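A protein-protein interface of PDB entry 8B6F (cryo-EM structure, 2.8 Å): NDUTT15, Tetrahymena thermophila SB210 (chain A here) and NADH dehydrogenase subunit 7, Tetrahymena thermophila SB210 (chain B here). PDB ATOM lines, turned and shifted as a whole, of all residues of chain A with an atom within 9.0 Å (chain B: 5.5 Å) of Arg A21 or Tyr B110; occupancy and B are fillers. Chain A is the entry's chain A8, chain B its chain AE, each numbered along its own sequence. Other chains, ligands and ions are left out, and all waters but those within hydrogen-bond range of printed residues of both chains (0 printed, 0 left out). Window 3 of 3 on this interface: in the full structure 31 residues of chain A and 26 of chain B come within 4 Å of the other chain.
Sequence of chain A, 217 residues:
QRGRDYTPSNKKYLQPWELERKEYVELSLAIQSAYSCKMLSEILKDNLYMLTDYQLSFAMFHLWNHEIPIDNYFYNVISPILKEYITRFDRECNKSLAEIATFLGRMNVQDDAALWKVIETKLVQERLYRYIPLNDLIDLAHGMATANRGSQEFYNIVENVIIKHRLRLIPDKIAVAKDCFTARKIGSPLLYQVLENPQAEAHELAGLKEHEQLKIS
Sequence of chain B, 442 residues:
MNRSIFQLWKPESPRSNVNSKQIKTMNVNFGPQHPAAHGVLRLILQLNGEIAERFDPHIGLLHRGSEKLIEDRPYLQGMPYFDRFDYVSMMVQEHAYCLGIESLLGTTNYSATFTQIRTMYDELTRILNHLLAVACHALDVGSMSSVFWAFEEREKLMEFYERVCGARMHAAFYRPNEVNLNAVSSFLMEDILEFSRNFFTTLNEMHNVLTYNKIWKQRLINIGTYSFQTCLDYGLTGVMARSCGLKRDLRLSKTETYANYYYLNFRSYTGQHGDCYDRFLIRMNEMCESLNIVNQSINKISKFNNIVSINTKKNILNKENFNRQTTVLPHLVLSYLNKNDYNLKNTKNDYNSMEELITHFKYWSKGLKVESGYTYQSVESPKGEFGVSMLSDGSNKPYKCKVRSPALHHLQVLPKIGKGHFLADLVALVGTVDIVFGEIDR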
ATOM      1  N   GLN A   1     -24.848  -0.238   1.751  1.00  0.00           N
ATOM      2  CA  GLN A   1     -26.000  -0.080   2.683  1.00  0.00           C
ATOM      3  C   GLN A   1     -26.640  -1.432   2.968  1.00  0.00           C
ATOM      4  O   GLN A   1     -26.378  -2.408   2.268  1.00  0.00           O
ATOM      5  CB  GLN A   1     -27.037   0.883   2.100  1.00  0.00           C
ATOM      6  CG  GLN A   1     -26.495   2.279   1.823  1.00  0.00           C
ATOM      7  CD  GLN A   1     -26.035   2.987   3.081  1.00  0.00           C
ATOM      8  OE1 GLN A   1     -26.414   2.616   4.190  1.00  0.00           O
ATOM      9  NE2 GLN A   1     -25.208   4.010   2.913  1.00  0.00           N
ATOM     10  N   ARG A   4     -29.394  -3.495   0.279  1.00  0.00           N
ATOM     11  CA  ARG A   4     -29.344  -2.634  -0.893  1.00  0.00           C
ATOM     12  C   ARG A   4     -28.692  -3.391  -2.039  1.00  0.00           C
ATOM     13  O   ARG A   4     -27.645  -4.021  -1.859  1.00  0.00           O
ATOM     14  CB  ARG A   4     -28.565  -1.351  -0.591  1.00  0.00           C
ATOM     15  CG  ARG A   4     -28.599  -0.316  -1.703  1.00  0.00           C
ATOM     16  CD  ARG A   4     -29.999   0.241  -1.906  1.00  0.00           C
ATOM     17  NE  ARG A   4     -29.993   1.395  -2.797  1.00  0.00           N
ATOM     18  CZ  ARG A   4     -29.997   1.323  -4.121  1.00  0.00           C
ATOM     19  NH1 ARG A   4     -30.012   0.160  -4.752  1.00  0.00           N
ATOM     20  NH2 ARG A   4     -29.985   2.447  -4.831  1.00  0.00           N
ATOM     21  N   GLN A  15     -27.729   5.075 -12.282  1.00  0.00           N
ATOM     22  CA  GLN A  15     -28.210   6.440 -12.404  1.00  0.00           C
ATOM     23  C   GLN A  15     -28.203   7.128 -11.047  1.00  0.00           C
ATOM     24  O   GLN A  15     -28.349   6.473 -10.012  1.00  0.00           O
ATOM     25  CB  GLN A  15     -29.629   6.473 -12.990  1.00  0.00           C
ATOM     26  CG  GLN A  15     -29.681   6.118 -14.466  1.00  0.00           C
ATOM     27  CD  GLN A  15     -31.096   6.035 -14.993  1.00  0.00           C
ATOM     28  OE1 GLN A  15     -32.024   5.695 -14.263  1.00  0.00           O
ATOM     29  NE2 GLN A  15     -31.268   6.351 -16.270  1.00  0.00           N
ATOM     30  N   PRO A  16     -28.036   8.454 -11.025  1.00  0.00           N
ATOM     31  CA  PRO A  16     -27.904   9.144  -9.732  1.00  0.00           C
ATOM     32  C   PRO A  16     -29.111   8.986  -8.824  1.00  0.00           C
ATOM     33  O   PRO A  16     -28.948   8.903  -7.601  1.00  0.00           O
ATOM     34  CB  PRO A  16     -27.684  10.607 -10.143  1.00  0.00           C
ATOM     35  CG  PRO A  16     -28.264  10.715 -11.505  1.00  0.00           C
ATOM     36  CD  PRO A  16     -28.015   9.394 -12.157  1.00  0.00           C
ATOM     37  N   TRP A  17     -30.322   8.940  -9.382  1.00  0.00           N
ATOM     38  CA  TRP A  17     -31.509   8.865  -8.539  1.00  0.00           C
ATOM     39  C   TRP A  17     -31.656   7.511  -7.862  1.00  0.00           C
ATOM     40  O   TRP A  17     -32.374   7.410  -6.864  1.00  0.00           O
ATOM     41  CB  TRP A  17     -32.764   9.180  -9.357  1.00  0.00           C
ATOM     42  CG  TRP A  17     -32.996   8.266 -10.518  1.00  0.00           C
ATOM     43  CD1 TRP A  17     -32.654   8.495 -11.817  1.00  0.00           C
ATOM     44  CD2 TRP A  17     -33.632   6.982 -10.491  1.00  0.00           C
ATOM     45  NE1 TRP A  17     -33.033   7.432 -12.600  1.00  0.00           N
ATOM     46  CE2 TRP A  17     -33.635   6.490 -11.810  1.00  0.00           C
ATOM     47  CE3 TRP A  17     -34.195   6.200  -9.477  1.00  0.00           C
ATOM     48  CZ2 TRP A  17     -34.178   5.252 -12.143  1.00  0.00           C
ATOM     49  CZ3 TRP A  17     -34.735   4.968  -9.811  1.00  0.00           C
ATOM     50  CH2 TRP A  17     -34.723   4.507 -11.134  1.00  0.00           C
ATOM     51  N   GLU A  18     -30.998   6.471  -8.378  1.00  0.00           N
ATOM     52  CA  GLU A  18     -31.046   5.173  -7.713  1.00  0.00           C
ATOM     53  C   GLU A  18     -30.309   5.209  -6.382  1.00  0.00           C
ATOM     54  O   GLU A  18     -30.759   4.612  -5.398  1.00  0.00           O
ATOM     55  CB  GLU A  18     -30.457   4.096  -8.621  1.00  0.00           C
ATOM     56  CG  GLU A  18     -31.142   3.995  -9.972  1.00  0.00           C
ATOM     57  CD  GLU A  18     -30.678   2.795 -10.768  1.00  0.00           C
ATOM     58  OE1 GLU A  18     -30.095   1.872 -10.164  1.00  0.00           O
ATOM     59  OE2 GLU A  18     -30.896   2.773 -11.997  1.00  0.00           O
ATOM     60  N   LEU A  19     -29.172   5.896  -6.333  1.00  0.00           N
ATOM     61  CA  LEU A  19     -28.408   6.017  -5.105  1.00  0.00           C
ATOM     62  C   LEU A  19     -29.044   7.044  -4.175  1.00  0.00           C
ATOM     63  O   LEU A  19     -29.784   7.934  -4.601  1.00  0.00           O
ATOM     64  CB  LEU A  19     -26.967   6.423  -5.407  1.00  0.00           C
ATOM     65  CG  LEU A  19     -26.156   5.458  -6.269  1.00  0.00           C
ATOM     66  CD1 LEU A  19     -24.831   6.089  -6.646  1.00  0.00           C
ATOM     67  CD2 LEU A  19     -25.937   4.141  -5.541  1.00  0.00           C
ATOM     68  N   GLU A  20     -28.740   6.913  -2.889  1.00  0.00           N
ATOM     69  CA  GLU A  20     -29.134   7.929  -1.928  1.00  0.00           C
ATOM     70  C   GLU A  20     -28.381   9.224  -2.202  1.00  0.00           C
ATOM     71  O   GLU A  20     -27.237   9.220  -2.663  1.00  0.00           O
ATOM     72  CB  GLU A  20     -28.859   7.458  -0.501  1.00  0.00           C
ATOM     73  CG  GLU A  20     -29.706   6.272  -0.077  1.00  0.00           C
ATOM     74  CD  GLU A  20     -29.456   5.864   1.359  1.00  0.00           C
ATOM     75  OE1 GLU A  20     -28.598   6.492   2.014  1.00  0.00           O
ATOM     76  OE2 GLU A  20     -30.115   4.916   1.834  1.00  0.00           O
ATOM     77  N   ARG A  21     -29.043  10.347  -1.921  1.00  0.00           N
ATOM     78  CA  ARG A  21     -28.428  11.640  -2.191  1.00  0.00           C
ATOM     79  C   ARG A  21     -27.143  11.808  -1.391  1.00  0.00           C
ATOM     80  O   ARG A  21     -26.165  12.376  -1.886  1.00  0.00           O
ATOM     81  CB  ARG A  21     -29.416  12.763  -1.875  1.00  0.00           C
ATOM     82  CG  ARG A  21     -29.003  14.138  -2.386  1.00  0.00           C
ATOM     83  CD  ARG A  21     -28.773  14.151  -3.892  1.00  0.00           C
ATOM     84  NE  ARG A  21     -29.795  13.408  -4.620  1.00  0.00           N
ATOM     85  CZ  ARG A  21     -30.961  13.905  -5.009  1.00  0.00           C
ATOM     86  NH1 ARG A  21     -31.305  15.153  -4.746  1.00  0.00           N
ATOM     87  NH2 ARG A  21     -31.805  13.127  -5.682  1.00  0.00           N
ATOM     88  N   LYS A  22     -27.122  11.310  -0.154  1.00  0.00           N
ATOM     89  CA  LYS A  22     -25.927  11.440   0.671  1.00  0.00           C
ATOM     90  C   LYS A  22     -24.741  10.734   0.027  1.00  0.00           C
ATOM     91  O   LYS A  22     -23.632  11.278  -0.023  1.00  0.00           O
ATOM     92  CB  LYS A  22     -26.192  10.880   2.067  1.00  0.00           C
ATOM     93  CG  LYS A  22     -27.078  11.762   2.928  1.00  0.00           C
ATOM     94  CD  LYS A  22     -27.178  11.217   4.343  1.00  0.00           C
ATOM     95  CE  LYS A  22     -27.974  12.143   5.243  1.00  0.00           C
ATOM     96  NZ  LYS A  22     -27.296  13.454   5.437  1.00  0.00           N
ATOM     97  N   GLU A  23     -24.952   9.511  -0.464  1.00  0.00           N
ATOM     98  CA  GLU A  23     -23.862   8.772  -1.092  1.00  0.00           C
ATOM     99  C   GLU A  23     -23.352   9.497  -2.330  1.00  0.00           C
ATOM    100  O   GLU A  23     -22.140   9.624  -2.536  1.00  0.00           O
ATOM    101  CB  GLU A  23     -24.322   7.361  -1.454  1.00  0.00           C
ATOM    102  CG  GLU A  23     -24.531   6.457  -0.260  1.00  0.00           C
ATOM    103  CD  GLU A  23     -24.841   5.033  -0.668  1.00  0.00           C
ATOM    104  OE1 GLU A  23     -25.408   4.840  -1.763  1.00  0.00           O
ATOM    105  OE2 GLU A  23     -24.504   4.105   0.098  1.00  0.00           O
ATOM    106  N   TYR A  24     -24.268   9.974  -3.172  1.00  0.00           N
ATOM    107  CA  TYR A  24     -23.869  10.671  -4.389  1.00  0.00           C
ATOM    108  C   TYR A  24     -23.051  11.914  -4.062  1.00  0.00           C
ATOM    109  O   TYR A  24     -21.994  12.154  -4.655  1.00  0.00           O
ATOM    110  CB  TYR A  24     -25.113  11.036  -5.199  1.00  0.00           C
ATOM    111  CG  TYR A  24     -24.828  11.601  -6.569  1.00  0.00           C
ATOM    112  CD1 TYR A  24     -24.572  10.764  -7.646  1.00  0.00           C
ATOM    113  CD2 TYR A  24     -24.846  12.970  -6.794  1.00  0.00           C
ATOM    114  CE1 TYR A  24     -24.322  11.273  -8.901  1.00  0.00           C
ATOM    115  CE2 TYR A  24     -24.596  13.489  -8.046  1.00  0.00           C
ATOM    116  CZ  TYR A  24     -24.337  12.634  -9.096  1.00  0.00           C
ATOM    117  OH  TYR A  24     -24.090  13.146 -10.346  1.00  0.00           O
ATOM    118  N   VAL A  25     -23.532  12.721  -3.116  1.00  0.00           N
ATOM    119  CA  VAL A  25     -22.843  13.960  -2.770  1.00  0.00           C
ATOM    120  C   VAL A  25     -21.473  13.666  -2.174  1.00  0.00           C
ATOM    121  O   VAL A  25     -20.481  14.324  -2.509  1.00  0.00           O
ATOM    122  CB  VAL A  25     -23.708  14.799  -1.812  1.00  0.00           C
ATOM    123  CG1 VAL A  25     -22.954  16.031  -1.350  1.00  0.00           C
ATOM    124  CG2 VAL A  25     -25.003  15.207  -2.489  1.00  0.00           C
ATOM    125  N   GLU A  26     -21.391  12.678  -1.282  1.00  0.00           N
ATOM    126  CA  GLU A  26     -20.117  12.388  -0.633  1.00  0.00           C
ATOM    127  C   GLU A  26     -19.096  11.842  -1.621  1.00  0.00           C
ATOM    128  O   GLU A  26     -17.917  12.204  -1.564  1.00  0.00           O
ATOM    129  CB  GLU A  26     -20.322  11.412   0.521  1.00  0.00           C
ATOM    130  CG  GLU A  26     -19.080  11.249   1.367  1.00  0.00           C
ATOM    131  CD  GLU A  26     -19.373  10.715   2.753  1.00  0.00           C
ATOM    132  OE1 GLU A  26     -20.549  10.413   3.041  1.00  0.00           O
ATOM    133  OE2 GLU A  26     -18.424  10.603   3.557  1.00  0.00           O
ATOM    134  N   LEU A  27     -19.522  10.965  -2.531  1.00  0.00           N
ATOM    135  CA  LEU A  27     -18.594  10.459  -3.536  1.00  0.00           C
ATOM    136  C   LEU A  27     -18.128  11.579  -4.455  1.00  0.00           C
ATOM    137  O   LEU A  27     -16.956  11.624  -4.847  1.00  0.00           O
ATOM    138  CB  LEU A  27     -19.238   9.325  -4.334  1.00  0.00           C
ATOM    139  CG  LEU A  27     -18.336   8.616  -5.351  1.00  0.00           C
ATOM    140  CD1 LEU A  27     -17.051   8.125  -4.715  1.00  0.00           C
ATOM    141  CD2 LEU A  27     -19.071   7.444  -5.972  1.00  0.00           C
ATOM    142  N   SER A  28     -19.032  12.493  -4.812  1.00  0.00           N
ATOM    143  CA  SER A  28     -18.638  13.634  -5.630  1.00  0.00           C
ATOM    144  C   SER A  28     -17.621  14.504  -4.902  1.00  0.00           C
ATOM    145  O   SER A  28     -16.649  14.973  -5.504  1.00  0.00           O
ATOM    146  CB  SER A  28     -19.870  14.454  -6.006  1.00  0.00           C
ATOM    147  OG  SER A  28     -20.863  13.637  -6.600  1.00  0.00           O
ATOM    148  N   LEU A  29     -17.829  14.734  -3.605  1.00  0.00           N
ATOM    149  CA  LEU A  29     -16.875  15.527  -2.835  1.00  0.00           C
ATOM    150  C   LEU A  29     -15.516  14.841  -2.773  1.00  0.00           C
ATOM    151  O   LEU A  29     -14.475  15.499  -2.872  1.00  0.00           O
ATOM    152  CB  LEU A  29     -17.412  15.781  -1.427  1.00  0.00           C
ATOM    153  CG  LEU A  29     -18.609  16.727  -1.299  1.00  0.00           C
ATOM    154  CD1 LEU A  29     -19.034  16.838   0.152  1.00  0.00           C
ATOM    155  CD2 LEU A  29     -18.292  18.103  -1.863  1.00  0.00           C
ATOM    156  N   GLN A  55     -20.281  11.307 -12.484  1.00  0.00           N
ATOM    157  CA  GLN A  55     -19.151  11.482 -11.581  1.00  0.00           C
ATOM    158  C   GLN A  55     -17.832  11.125 -12.248  1.00  0.00           C
ATOM    159  O   GLN A  55     -16.806  11.751 -11.961  1.00  0.00           O
ATOM    160  CB  GLN A  55     -19.361  10.644 -10.324  1.00  0.00           C
ATOM    161  CG  GLN A  55     -20.532  11.109  -9.479  1.00  0.00           C
ATOM    162  CD  GLN A  55     -20.714  10.260  -8.249  1.00  0.00           C
ATOM    163  OE1 GLN A  55     -20.174   9.163  -8.163  1.00  0.00           O
ATOM    164  NE2 GLN A  55     -21.468  10.764  -7.284  1.00  0.00           N
ATOM    165  N   THR B 108     -30.525  15.500   2.000  1.00  0.00           N
ATOM    166  CA  THR B 108     -29.411  16.412   2.206  1.00  0.00           C
ATOM    167  C   THR B 108     -29.510  17.537   1.189  1.00  0.00           C
ATOM    168  O   THR B 108     -30.111  17.388   0.123  1.00  0.00           O
ATOM    169  CB  THR B 108     -28.057  15.696   2.081  1.00  0.00           C
ATOM    170  OG1 THR B 108     -26.993  16.614   2.359  1.00  0.00           O
ATOM    171  CG2 THR B 108     -27.873  15.121   0.684  1.00  0.00           C
ATOM    172  N   ASN B 109     -28.914  18.678   1.536  1.00  0.00           N
ATOM    173  CA  ASN B 109     -28.948  19.861   0.676  1.00  0.00           C
ATOM    174  C   ASN B 109     -27.790  19.774  -0.312  1.00  0.00           C
ATOM    175  O   ASN B 109     -26.729  20.377  -0.143  1.00  0.00           O
ATOM    176  CB  ASN B 109     -28.894  21.133   1.510  1.00  0.00           C
ATOM    177  CG  ASN B 109     -29.240  22.366   0.708  1.00  0.00           C
ATOM    178  OD1 ASN B 109     -29.486  22.286  -0.494  1.00  0.00           O
ATOM    179  ND2 ASN B 109     -29.281  23.513   1.372  1.00  0.00           N
ATOM    180  N   TYR B 110     -28.010  18.993  -1.370  1.00  0.00           N
ATOM    181  CA  TYR B 110     -26.986  18.824  -2.395  1.00  0.00           C
ATOM    182  C   TYR B 110     -26.668  20.146  -3.080  1.00  0.00           C
ATOM    183  O   TYR B 110     -25.510  20.415  -3.420  1.00  0.00           O
ATOM    184  CB  TYR B 110     -27.436  17.785  -3.421  1.00  0.00           C
ATOM    185  CG  TYR B 110     -28.663  18.188  -4.204  1.00  0.00           C
ATOM    186  CD1 TYR B 110     -29.935  18.006  -3.680  1.00  0.00           C
ATOM    187  CD2 TYR B 110     -28.550  18.743  -5.471  1.00  0.00           C
ATOM    188  CE1 TYR B 110     -31.058  18.370  -4.390  1.00  0.00           C
ATOM    189  CE2 TYR B 110     -29.669  19.111  -6.190  1.00  0.00           C
ATOM    190  CZ  TYR B 110     -30.920  18.922  -5.644  1.00  0.00           C
ATOM    191  OH  TYR B 110     -32.038  19.285  -6.353  1.00  0.00           O
ATOM    192  N   SER B 111     -27.681  20.990  -3.285  1.00  0.00           N
ATOM    193  CA  SER B 111     -27.447  22.283  -3.920  1.00  0.00           C
ATOM    194  C   SER B 111     -26.452  23.110  -3.119  1.00  0.00           C
ATOM    195  O   SER B 111     -25.473  23.628  -3.667  1.00  0.00           O
ATOM    196  CB  SER B 111     -28.768  23.038  -4.073  1.00  0.00           C
ATOM    197  OG  SER B 111     -29.707  22.278  -4.812  1.00  0.00           O
ATOM    198  N   ALA B 112     -26.691  23.251  -1.816  1.00  0.00           N
ATOM    199  CA  ALA B 112     -25.766  24.009  -0.982  1.00  0.00           C
ATOM    200  C   ALA B 112     -24.395  23.347  -0.935  1.00  0.00           C
ATOM    201  O   ALA B 112     -23.367  24.030  -0.986  1.00  0.00           O
ATOM    202  CB  ALA B 112     -26.334  24.157   0.428  1.00  0.00           C
ATOM    203  N   THR B 113     -24.359  22.017  -0.825  1.00  0.00           N
ATOM    204  CA  THR B 113     -23.078  21.325  -0.737  1.00  0.00           C
ATOM    205  C   THR B 113     -22.237  21.557  -1.985  1.00  0.00           C
ATOM    206  O   THR B 113     -21.033  21.821  -1.891  1.00  0.00           O
ATOM    207  CB  THR B 113     -23.297  19.830  -0.518  1.00  0.00           C
ATOM    208  OG1 THR B 113     -24.117  19.625   0.640  1.00  0.00           O
ATOM    209  CG2 THR B 113     -21.966  19.127  -0.309  1.00  0.00           C
ATOM    210  N   PHE B 114     -22.852  21.466  -3.166  1.00  0.00           N
ATOM    211  CA  PHE B 114     -22.105  21.642  -4.406  1.00  0.00           C
ATOM    212  C   PHE B 114     -21.793  23.104  -4.690  1.00  0.00           C
ATOM    213  O   PHE B 114     -20.786  23.401  -5.341  1.00  0.00           O
ATOM    214  CB  PHE B 114     -22.876  21.030  -5.578  1.00  0.00           C
ATOM    215  CG  PHE B 114     -22.976  19.527  -5.526  1.00  0.00           C
ATOM    216  CD1 PHE B 114     -21.933  18.762  -5.024  1.00  0.00           C
ATOM    217  CD2 PHE B 114     -24.112  18.881  -5.981  1.00  0.00           C
ATOM    218  CE1 PHE B 114     -22.024  17.386  -4.976  1.00  0.00           C
ATOM    219  CE2 PHE B 114     -24.207  17.502  -5.936  1.00  0.00           C
ATOM    220  CZ  PHE B 114     -23.162  16.756  -5.434  1.00  0.00           C
ATOM    221  N   THR B 115     -22.632  24.027  -4.222  1.00  0.00           N
ATOM    222  CA  THR B 115     -22.338  25.444  -4.386  1.00  0.00           C
ATOM    223  C   THR B 115     -21.316  25.949  -3.378  1.00  0.00           C
ATOM    224  O   THR B 115     -20.764  27.037  -3.571  1.00  0.00           O
ATOM    225  CB  THR B 115     -23.623  26.264  -4.262  1.00  0.00           C
ATOM    226  OG1 THR B 115     -24.674  25.622  -4.994  1.00  0.00           O
ATOM    227  CG2 THR B 115     -23.419  27.665  -4.815  1.00  0.00           C
ATOM    228  N   LEU B 334     -22.620  22.111  -9.578  1.00  0.00           N
ATOM    229  CA  LEU B 334     -24.041  21.781  -9.529  1.00  0.00           C
ATOM    230  C   LEU B 334     -24.577  21.474 -10.921  1.00  0.00           C
ATOM    231  O   LEU B 334     -25.280  20.479 -11.123  1.00  0.00           O
ATOM    232  CB  LEU B 334     -24.823  22.928  -8.889  1.00  0.00           C
ATOM    233  CG  LEU B 334     -26.316  22.679  -8.667  1.00  0.00           C
ATOM    234  CD1 LEU B 334     -26.537  21.562  -7.664  1.00  0.00           C
ATOM    235  CD2 LEU B 334     -27.004  23.951  -8.209  1.00  0.00           C
ATOM    236  N   ASN B 338     -25.756  17.615 -11.104  1.00  0.00           N
ATOM    237  CA  ASN B 338     -27.218  17.578 -11.071  1.00  0.00           C
ATOM    238  C   ASN B 338     -27.776  18.460 -12.186  1.00  0.00           C
ATOM    239  O   ASN B 338     -28.284  19.560 -11.967  1.00  0.00           O
ATOM    240  CB  ASN B 338     -27.731  18.014  -9.702  1.00  0.00           C
ATOM    241  CG  ASN B 338     -27.412  17.011  -8.615  1.00  0.00           C
ATOM    242  OD1 ASN B 338     -26.348  17.058  -8.003  1.00  0.00           O
ATOM    243  ND2 ASN B 338     -28.340  16.093  -8.368  1.00  0.00           N
ATOM    244  N   ASP B 341     -31.879  18.409 -12.169  1.00  0.00           N
ATOM    245  CA  ASP B 341     -32.409  19.225 -11.083  1.00  0.00           C
ATOM    246  C   ASP B 341     -32.174  20.704 -11.351  1.00  0.00           C
ATOM    247  O   ASP B 341     -33.061  21.535 -11.121  1.00  0.00           O
ATOM    248  CB  ASP B 341     -31.768  18.808  -9.761  1.00  0.00           C
ATOM    249  CG  ASP B 341     -31.905  17.324  -9.489  1.00  0.00           C
ATOM    250  OD1 ASP B 341     -32.975  16.760  -9.800  1.00  0.00           O
ATOM    251  OD2 ASP B 341     -30.941  16.720  -8.975  1.00  0.00           O
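Printed residues of chain B within 4 Å of Arg A21: Thr B108 (3.4 Å) and Tyr B110 (3.2 Å).
Of chain A, only Arg A21 and Val A25 come within 4 Å of Tyr B110.
No residue of chain A comes within 4 Å of Ser B111.
Thr B113 touches just these residues of chain A: Val A25 (3.4 Å) and Leu A29 (3.7 Å).
Of the printed residues of chain B, Leu A29 touches Thr B113 (3.7 Å).
Printed residues of chain B within 4 Å of Lys A22: Thr B108.
The nearest printed residue of chain B that does not touch Lys A22 is Asn B109 (6.7 Å).
Of the 11 printed residues of chain B, 5 touch a printed residue of chain A.
Along chain B the printed residues that touch a printed residue of chain A span positions 108 to 338.
Hydrophobic or aromatic side chains of chain A that line the printed part of chain B: Tyr A24, Val A25 and Leu A29.
Among the printed residues, 9 pairs touch across the chains.
Among the printed residues, merely in contact across the chains: Arg A21 with Tyr B110, Val A25 with Thr B113, Arg A21 with Thr B108, Val A25 with Tyr B110, Leu A29 with Thr B113, Ser A28 with Phe B114, Val A25 with Phe B114, Lys A22 with Thr B108 and Tyr A24 with Asn B338.
The side-chain hydroxyl (OG) of Ser A28 sits at hydrogen-bond distance from the side-chain amide nitrogen (NE2) of Gln A55, 3.0 Å away.
The backbone carbonyl oxygen (O) of Tyr A24 is in hydrogen-bond range of the side-chain hydroxyl (OG) of Ser A28 (2.7 Å).
The side-chain carboxylate of Asp B341 sits at hydrogen-bond distance from the side-chain amide nitrogen of Asn B338.
The side-chain amide nitrogen of Gln A55 is in hydrogen-bond range of the backbone carbonyl oxygen of Tyr A24 (3.0 Å).
The backbone carbonyl oxygen (O) of Asn B109 is in hydrogen-bond range of the side-chain hydroxyl (OG1) of Thr B113 (2.8 Å).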
